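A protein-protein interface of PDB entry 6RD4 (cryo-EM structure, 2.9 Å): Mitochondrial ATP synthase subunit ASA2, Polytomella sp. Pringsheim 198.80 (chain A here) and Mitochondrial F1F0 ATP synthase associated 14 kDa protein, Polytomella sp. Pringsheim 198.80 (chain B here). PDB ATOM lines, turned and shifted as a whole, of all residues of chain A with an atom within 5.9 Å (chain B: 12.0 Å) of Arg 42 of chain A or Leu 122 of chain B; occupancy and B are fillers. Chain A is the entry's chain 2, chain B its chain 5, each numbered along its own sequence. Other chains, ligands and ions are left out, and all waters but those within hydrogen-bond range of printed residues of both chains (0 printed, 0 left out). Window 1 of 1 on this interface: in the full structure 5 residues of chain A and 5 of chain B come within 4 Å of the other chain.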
ATOM      1  N   ASN A  40       7.737 -10.854  -9.800  1.00  0.00           N
ATOM      2  CA  ASN A  40       7.381 -11.883  -8.831  1.00  0.00           C
ATOM      3  C   ASN A  40       6.013 -11.537  -8.268  1.00  0.00           C
ATOM      4  O   ASN A  40       5.885 -10.654  -7.421  1.00  0.00           O
ATOM      5  CB  ASN A  40       8.427 -11.969  -7.733  1.00  0.00           C
ATOM      6  CG  ASN A  40       8.505 -13.332  -7.125  1.00  0.00           C
ATOM      7  OD1 ASN A  40       7.878 -14.269  -7.599  1.00  0.00           O
ATOM      8  ND2 ASN A  40       9.289 -13.459  -6.071  1.00  0.00           N
ATOM      9  N   ARG A  41       4.987 -12.229  -8.752  1.00  0.00           N
ATOM     10  CA  ARG A  41       3.636 -11.952  -8.304  1.00  0.00           C
ATOM     11  C   ARG A  41       3.302 -12.692  -7.031  1.00  0.00           C
ATOM     12  O   ARG A  41       2.499 -12.202  -6.237  1.00  0.00           O
ATOM     13  CB  ARG A  41       2.634 -12.342  -9.374  1.00  0.00           C
ATOM     14  CG  ARG A  41       2.893 -11.741 -10.704  1.00  0.00           C
ATOM     15  CD  ARG A  41       2.018 -12.405 -11.723  1.00  0.00           C
ATOM     16  NE  ARG A  41       0.643 -12.485 -11.270  1.00  0.00           N
ATOM     17  CZ  ARG A  41      -0.250 -11.530 -11.468  1.00  0.00           C
ATOM     18  NH1 ARG A  41      -1.487 -11.672 -11.031  1.00  0.00           N
ATOM     19  NH2 ARG A  41       0.100 -10.429 -12.113  1.00  0.00           N
ATOM     20  N   ARG A  42       3.887 -13.874  -6.831  1.00  0.00           N
ATOM     21  CA  ARG A  42       3.576 -14.653  -5.641  1.00  0.00           C
ATOM     22  C   ARG A  42       4.150 -13.999  -4.398  1.00  0.00           C
ATOM     23  O   ARG A  42       3.526 -14.030  -3.339  1.00  0.00           O
ATOM     24  CB  ARG A  42       4.092 -16.073  -5.808  1.00  0.00           C
ATOM     25  CG  ARG A  42       3.825 -17.007  -4.661  1.00  0.00           C
ATOM     26  CD  ARG A  42       2.386 -16.999  -4.225  1.00  0.00           C
ATOM     27  NE  ARG A  42       2.164 -17.858  -3.076  1.00  0.00           N
ATOM     28  CZ  ARG A  42       1.318 -17.577  -2.102  1.00  0.00           C
ATOM     29  NH1 ARG A  42       0.625 -16.464  -2.135  1.00  0.00           N
ATOM     30  NH2 ARG A  42       1.169 -18.403  -1.092  1.00  0.00           N
ATOM     31  N   LEU A  43       5.311 -13.368  -4.514  1.00  0.00           N
ATOM     32  CA  LEU A  43       5.878 -12.661  -3.375  1.00  0.00           C
ATOM     33  C   LEU A  43       5.065 -11.433  -3.021  1.00  0.00           C
ATOM     34  O   LEU A  43       4.971 -11.073  -1.848  1.00  0.00           O
ATOM     35  CB  LEU A  43       7.319 -12.277  -3.672  1.00  0.00           C
ATOM     36  CG  LEU A  43       8.125 -11.523  -2.629  1.00  0.00           C
ATOM     37  CD1 LEU A  43       8.030 -12.207  -1.304  1.00  0.00           C
ATOM     38  CD2 LEU A  43       9.540 -11.461  -3.091  1.00  0.00           C
ATOM     39  N   TRP A  44       4.456 -10.788  -4.005  1.00  0.00           N
ATOM     40  CA  TRP A  44       3.525  -9.723  -3.681  1.00  0.00           C
ATOM     41  C   TRP A  44       2.235 -10.285  -3.122  1.00  0.00           C
ATOM     42  O   TRP A  44       1.539  -9.604  -2.369  1.00  0.00           O
ATOM     43  CB  TRP A  44       3.233  -8.885  -4.908  1.00  0.00           C
ATOM     44  CG  TRP A  44       3.978  -7.627  -4.989  1.00  0.00           C
ATOM     45  CD1 TRP A  44       4.899  -7.302  -5.914  1.00  0.00           C
ATOM     46  CD2 TRP A  44       3.854  -6.500  -4.126  1.00  0.00           C
ATOM     47  NE1 TRP A  44       5.370  -6.044  -5.685  1.00  0.00           N
ATOM     48  CE2 TRP A  44       4.740  -5.529  -4.589  1.00  0.00           C
ATOM     49  CE3 TRP A  44       3.088  -6.221  -3.001  1.00  0.00           C
ATOM     50  CZ2 TRP A  44       4.872  -4.306  -3.980  1.00  0.00           C
ATOM     51  CZ3 TRP A  44       3.230  -5.007  -2.394  1.00  0.00           C
ATOM     52  CH2 TRP A  44       4.106  -4.065  -2.886  1.00  0.00           C
ATOM     53  N   GLY A  45       1.909 -11.525  -3.471  1.00  0.00           N
ATOM     54  CA  GLY A  45       0.728 -12.149  -2.921  1.00  0.00           C
ATOM     55  C   GLY A  45       0.893 -12.566  -1.482  1.00  0.00           C
ATOM     56  O   GLY A  45      -0.065 -12.524  -0.715  1.00  0.00           O
ATOM     57  N   LYS A  46       2.097 -12.976  -1.088  1.00  0.00           N
ATOM     58  CA  LYS A  46       2.322 -13.332   0.306  1.00  0.00           C
ATOM     59  C   LYS A  46       2.302 -12.112   1.202  1.00  0.00           C
ATOM     60  O   LYS A  46       2.036 -12.230   2.396  1.00  0.00           O
ATOM     61  CB  LYS A  46       3.654 -14.041   0.473  1.00  0.00           C
ATOM     62  CG  LYS A  46       3.828 -15.287  -0.321  1.00  0.00           C
ATOM     63  CD  LYS A  46       4.886 -16.140   0.302  1.00  0.00           C
ATOM     64  CE  LYS A  46       5.326 -17.240  -0.619  1.00  0.00           C
ATOM     65  NZ  LYS A  46       6.328 -16.760  -1.597  1.00  0.00           N
ATOM     66  N   VAL A  47       2.612 -10.942   0.661  1.00  0.00           N
ATOM     67  CA  VAL A  47       2.607  -9.732   1.465  1.00  0.00           C
ATOM     68  C   VAL A  47       1.190  -9.253   1.689  1.00  0.00           C
ATOM     69  O   VAL A  47       0.823  -8.867   2.799  1.00  0.00           O
ATOM     70  CB  VAL A  47       3.481  -8.658   0.802  1.00  0.00           C
ATOM     71  CG1 VAL A  47       3.380  -7.361   1.530  1.00  0.00           C
ATOM     72  CG2 VAL A  47       4.901  -9.104   0.786  1.00  0.00           C
ATOM     73  N   LEU A  48       0.352  -9.291   0.658  1.00  0.00           N
ATOM     74  CA  LEU A  48      -1.020  -8.869   0.864  1.00  0.00           C
ATOM     75  C   LEU A  48      -1.842  -9.926   1.575  1.00  0.00           C
ATOM     76  O   LEU A  48      -2.912  -9.612   2.088  1.00  0.00           O
ATOM     77  CB  LEU A  48      -1.669  -8.494  -0.460  1.00  0.00           C
ATOM     78  CG  LEU A  48      -1.123  -7.247  -1.143  1.00  0.00           C
ATOM     79  CD1 LEU A  48      -1.985  -6.884  -2.297  1.00  0.00           C
ATOM     80  CD2 LEU A  48      -1.041  -6.092  -0.190  1.00  0.00           C
ATOM     81  N   GLU A  49      -1.379 -11.167   1.618  1.00  0.00           N
ATOM     82  CA  GLU A  49      -2.041 -12.158   2.453  1.00  0.00           C
ATOM     83  C   GLU A  49      -1.821 -11.871   3.923  1.00  0.00           C
ATOM     84  O   GLU A  49      -2.732 -12.041   4.733  1.00  0.00           O
ATOM     85  CB  GLU A  49      -1.531 -13.543   2.119  1.00  0.00           C
ATOM     86  CG  GLU A  49      -2.315 -14.214   1.064  1.00  0.00           C
ATOM     87  CD  GLU A  49      -1.945 -15.653   0.944  1.00  0.00           C
ATOM     88  OE1 GLU A  49      -0.738 -15.948   0.897  1.00  0.00           O
ATOM     89  OE2 GLU A  49      -2.865 -16.494   0.913  1.00  0.00           O
ATOM     90  N   HIS A  76      -5.333  -5.626  -5.222  1.00  0.00           N
ATOM     91  CA  HIS A  76      -6.178  -6.725  -4.798  1.00  0.00           C
ATOM     92  C   HIS A  76      -7.269  -6.050  -3.999  1.00  0.00           C
ATOM     93  O   HIS A  76      -6.973  -5.491  -2.948  1.00  0.00           O
ATOM     94  CB  HIS A  76      -5.417  -7.734  -3.960  1.00  0.00           C
ATOM     95  CG  HIS A  76      -6.248  -8.894  -3.523  1.00  0.00           C
ATOM     96  ND1 HIS A  76      -6.478  -9.186  -2.201  1.00  0.00           N
ATOM     97  CD2 HIS A  76      -6.922  -9.821  -4.236  1.00  0.00           C
ATOM     98  CE1 HIS A  76      -7.252 -10.249  -2.116  1.00  0.00           C
ATOM     99  NE2 HIS A  76      -7.538 -10.651  -3.339  1.00  0.00           N
ATOM    100  N   THR A  79      -8.022  -7.039  -0.164  1.00  0.00           N
ATOM    101  CA  THR A  79      -7.031  -6.679   0.836  1.00  0.00           C
ATOM    102  C   THR A  79      -7.026  -5.192   1.107  1.00  0.00           C
ATOM    103  O   THR A  79      -6.986  -4.773   2.265  1.00  0.00           O
ATOM    104  CB  THR A  79      -5.659  -7.113   0.376  1.00  0.00           C
ATOM    105  OG1 THR A  79      -5.708  -8.492   0.008  1.00  0.00           O
ATOM    106  CG2 THR A  79      -4.680  -6.919   1.477  1.00  0.00           C
ATOM    107  N   LEU B 108       1.005 -28.132   7.736  1.00  0.00           N
ATOM    108  CA  LEU B 108       1.805 -27.431   6.707  1.00  0.00           C
ATOM    109  C   LEU B 108       2.867 -28.311   6.081  1.00  0.00           C
ATOM    110  O   LEU B 108       3.497 -27.873   5.139  1.00  0.00           O
ATOM    111  CB  LEU B 108       2.517 -26.147   7.159  1.00  0.00           C
ATOM    112  CG  LEU B 108       1.561 -25.070   7.631  1.00  0.00           C
ATOM    113  CD1 LEU B 108       2.310 -23.878   8.197  1.00  0.00           C
ATOM    114  CD2 LEU B 108       0.677 -24.671   6.480  1.00  0.00           C
ATOM    115  N   LEU B 114      -5.334 -28.409   4.813  1.00  0.00           N
ATOM    116  CA  LEU B 114      -6.458 -27.576   4.451  1.00  0.00           C
ATOM    117  C   LEU B 114      -6.082 -26.125   4.261  1.00  0.00           C
ATOM    118  O   LEU B 114      -6.982 -25.311   4.109  1.00  0.00           O
ATOM    119  CB  LEU B 114      -7.552 -27.655   5.506  1.00  0.00           C
ATOM    120  CG  LEU B 114      -8.198 -28.996   5.784  1.00  0.00           C
ATOM    121  CD1 LEU B 114      -9.506 -28.741   6.440  1.00  0.00           C
ATOM    122  CD2 LEU B 114      -8.396 -29.813   4.544  1.00  0.00           C
ATOM    123  N   ILE B 115      -4.802 -25.763   4.264  1.00  0.00           N
ATOM    124  CA  ILE B 115      -4.472 -24.347   4.259  1.00  0.00           C
ATOM    125  C   ILE B 115      -4.671 -23.728   2.887  1.00  0.00           C
ATOM    126  O   ILE B 115      -4.898 -22.524   2.783  1.00  0.00           O
ATOM    127  CB  ILE B 115      -3.044 -24.143   4.799  1.00  0.00           C
ATOM    128  CG1 ILE B 115      -2.777 -22.688   5.144  1.00  0.00           C
ATOM    129  CG2 ILE B 115      -2.021 -24.615   3.826  1.00  0.00           C
ATOM    130  CD1 ILE B 115      -3.666 -22.171   6.201  1.00  0.00           C
ATOM    131  N   TRP B 116      -4.659 -24.513   1.826  1.00  0.00           N
ATOM    132  CA  TRP B 116      -4.924 -23.975   0.509  1.00  0.00           C
ATOM    133  C   TRP B 116      -6.373 -24.121   0.139  1.00  0.00           C
ATOM    134  O   TRP B 116      -6.792 -23.615  -0.897  1.00  0.00           O
ATOM    135  CB  TRP B 116      -4.044 -24.661  -0.527  1.00  0.00           C
ATOM    136  CG  TRP B 116      -2.661 -24.786  -0.070  1.00  0.00           C
ATOM    137  CD1 TRP B 116      -2.035 -25.916   0.295  1.00  0.00           C
ATOM    138  CD2 TRP B 116      -1.724 -23.731   0.106  1.00  0.00           C
ATOM    139  NE1 TRP B 116      -0.762 -25.646   0.684  1.00  0.00           N
ATOM    140  CE2 TRP B 116      -0.549 -24.302   0.582  1.00  0.00           C
ATOM    141  CE3 TRP B 116      -1.769 -22.354  -0.094  1.00  0.00           C
ATOM    142  CZ2 TRP B 116       0.573 -23.556   0.851  1.00  0.00           C
ATOM    143  CZ3 TRP B 116      -0.660 -21.619   0.182  1.00  0.00           C
ATOM    144  CH2 TRP B 116       0.496 -22.214   0.649  1.00  0.00           C
ATOM    145  N   GLN B 117      -7.143 -24.805   0.963  1.00  0.00           N
ATOM    146  CA  GLN B 117      -8.564 -24.890   0.758  1.00  0.00           C
ATOM    147  C   GLN B 117      -9.331 -23.878   1.567  1.00  0.00           C
ATOM    148  O   GLN B 117     -10.438 -23.531   1.175  1.00  0.00           O
ATOM    149  CB  GLN B 117      -9.086 -26.266   1.136  1.00  0.00           C
ATOM    150  CG  GLN B 117      -8.256 -27.388   0.703  1.00  0.00           C
ATOM    151  CD  GLN B 117      -8.963 -28.673   0.918  1.00  0.00           C
ATOM    152  OE1 GLN B 117     -10.143 -28.687   1.207  1.00  0.00           O
ATOM    153  NE2 GLN B 117      -8.251 -29.767   0.792  1.00  0.00           N
ATOM    154  N   VAL B 118      -8.807 -23.423   2.694  1.00  0.00           N
ATOM    155  CA  VAL B 118      -9.549 -22.497   3.524  1.00  0.00           C
ATOM    156  C   VAL B 118      -9.041 -21.077   3.385  1.00  0.00           C
ATOM    157  O   VAL B 118      -9.826 -20.139   3.555  1.00  0.00           O
ATOM    158  CB  VAL B 118      -9.563 -22.936   5.005  1.00  0.00           C
ATOM    159  CG1 VAL B 118     -10.014 -24.344   5.118  1.00  0.00           C
ATOM    160  CG2 VAL B 118      -8.260 -22.760   5.682  1.00  0.00           C
ATOM    161  N   LYS B 119      -7.786 -20.882   3.028  1.00  0.00           N
ATOM    162  CA  LYS B 119      -7.219 -19.564   2.814  1.00  0.00           C
ATOM    163  C   LYS B 119      -6.531 -19.663   1.471  1.00  0.00           C
ATOM    164  O   LYS B 119      -5.349 -20.018   1.405  1.00  0.00           O
ATOM    165  CB  LYS B 119      -6.236 -19.188   3.911  1.00  0.00           C
ATOM    166  CG  LYS B 119      -6.869 -18.732   5.180  1.00  0.00           C
ATOM    167  CD  LYS B 119      -7.417 -17.355   5.032  1.00  0.00           C
ATOM    168  CE  LYS B 119      -8.113 -16.926   6.288  1.00  0.00           C
ATOM    169  NZ  LYS B 119      -8.785 -15.616   6.111  1.00  0.00           N
ATOM    170  N   PRO B 120      -7.241 -19.388   0.383  1.00  0.00           N
ATOM    171  CA  PRO B 120      -6.648 -19.551  -0.938  1.00  0.00           C
ATOM    172  C   PRO B 120      -5.555 -18.531  -1.195  1.00  0.00           C
ATOM    173  O   PRO B 120      -5.649 -17.373  -0.790  1.00  0.00           O
ATOM    174  CB  PRO B 120      -7.835 -19.351  -1.878  1.00  0.00           C
ATOM    175  CG  PRO B 120      -8.793 -18.618  -1.120  1.00  0.00           C
ATOM    176  CD  PRO B 120      -8.658 -19.033   0.283  1.00  0.00           C
ATOM    177  N   ALA B 121      -4.509 -18.989  -1.862  1.00  0.00           N
ATOM    178  CA  ALA B 121      -3.282 -18.230  -2.000  1.00  0.00           C
ATOM    179  C   ALA B 121      -3.442 -17.113  -3.009  1.00  0.00           C
ATOM    180  O   ALA B 121      -4.048 -17.302  -4.061  1.00  0.00           O
ATOM    181  CB  ALA B 121      -2.156 -19.152  -2.434  1.00  0.00           C
ATOM    182  N   LEU B 122      -2.875 -15.962  -2.700  1.00  0.00           N
ATOM    183  CA  LEU B 122      -2.837 -14.853  -3.633  1.00  0.00           C
ATOM    184  C   LEU B 122      -1.674 -15.035  -4.586  1.00  0.00           C
ATOM    185  O   LEU B 122      -0.517 -14.951  -4.179  1.00  0.00           O
ATOM    186  CB  LEU B 122      -2.692 -13.544  -2.881  1.00  0.00           C
ATOM    187  CG  LEU B 122      -3.996 -12.939  -2.455  1.00  0.00           C
ATOM    188  CD1 LEU B 122      -3.747 -11.772  -1.581  1.00  0.00           C
ATOM    189  CD2 LEU B 122      -4.651 -12.498  -3.681  1.00  0.00           C
ATOM    190  N   PHE B 123      -1.965 -15.262  -5.850  1.00  0.00           N
ATOM    191  CA  PHE B 123      -0.902 -15.423  -6.816  1.00  0.00           C
ATOM    192  C   PHE B 123      -0.769 -14.227  -7.739  1.00  0.00           C
ATOM    193  O   PHE B 123      -1.761 -13.661  -8.184  1.00  0.00           O
ATOM    194  CB  PHE B 123      -1.130 -16.682  -7.625  1.00  0.00           C
ATOM    195  CG  PHE B 123      -0.508 -17.879  -7.031  1.00  0.00           C
ATOM    196  CD1 PHE B 123       0.793 -18.198  -7.318  1.00  0.00           C
ATOM    197  CD2 PHE B 123      -1.207 -18.683  -6.174  1.00  0.00           C
ATOM    198  CE1 PHE B 123       1.374 -19.305  -6.769  1.00  0.00           C
ATOM    199  CE2 PHE B 123      -0.630 -19.791  -5.622  1.00  0.00           C
ATOM    200  CZ  PHE B 123       0.662 -20.099  -5.919  1.00  0.00           C
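The backbone carbonyl oxygen (O) of Phe 123 of chain B sits at hydrogen-bond distance from the guanidinium group (NH1) of Arg 41 of chain A, at 3.5 Å.
The guanidinium group of Arg 42 of chain A is in hydrogen-bond range of the backbone carbonyl oxygen of Leu 122 of chain B, 2.8 Å away.
The side-chain carboxylate of Glu 49 of chain A sits close to the backbone carbonyl oxygen of Pro 120 of chain B, at 3.4 Å.
The guanidinium group of Arg 42 of chain A is in salt-bridge range of the side-chain carboxylate of Glu 49 of chain A, 3.4 Å away.
OG1 of Thr 79 of chain A sits at hydrogen-bond distance from ND1 of His 76 of chain A, 2.4 Å away.
Arg 42 of chain A touches Trp 116 of chain B (NH2 to CZ3, 3.9 Å).
Arg 42 of chain A touches Ala 121 of chain B (NH2 to CB, 3.7 Å).
Arg 42 of chain A touches Phe 123 of chain B (CD to CE1, 3.6 Å).
Leu 122 of chain B touches Gly 45 of chain A.
Glu 49 of chain A touches Ala 121 of chain B (OE2 to CA, 3.4 Å).
Leu 122 of chain B touches Glu 49 of chain A.
NE2 of His 76 of chain A touches CD2 of Leu 122 of chain B, 3.4 Å away.
Of chain B, only Trp 116 (3.9 Å), Ala 121 (3.7 Å), Leu 122 (2.8 Å) and Phe 123 (3.6 Å) come within 4 Å of Arg 42 of chain A.
Of chain A, only Arg 42, Gly 45, Glu 49 and His 76 come within 4 Å of Leu 122 of chain B.
No residue of chain B comes within 4 Å of Leu 43 of chain A.
Gly 45 of chain A touches just one residue of chain B: Leu 122.
No residue of chain B comes within 4 Å of Lys 46 of chain A.
No residue of chain B comes within 4 Å of Leu 48 of chain A.
Glu 49 of chain A touches three residues of chain B.
His 76 of chain A touches just one residue of chain B: Leu 122 (3.4 Å).
Of the printed residues of chain A, Ala 121 of chain B touches Arg 42 (3.7 Å) and Glu 49 (3.4 Å).
Printed residues of chain A within 4 Å of Trp 116 of chain B: Arg 42.
Of the printed residues of chain A, Pro 120 of chain B touches Glu 49 (3.4 Å).
Of the printed residues of chain A, Phe 123 of chain B touches Arg 41 and Arg 42.
Val 118 of chain B touches none of the printed residues of chain A.
The nearest residue of chain A that does not touch Leu 122 of chain B is Leu 48 of chain A (4.04 Å).
Printed residues of chain B that touch a printed residue of chain A: Trp 116, Pro 120, Ala 121, Leu 122 and Phe 123.
Hydrophobic or aromatic side chains of chain A that line the printed part of chain B: His 76.
Along chain A the printed residues that touch a printed residue of chain B span positions 41 to 76.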
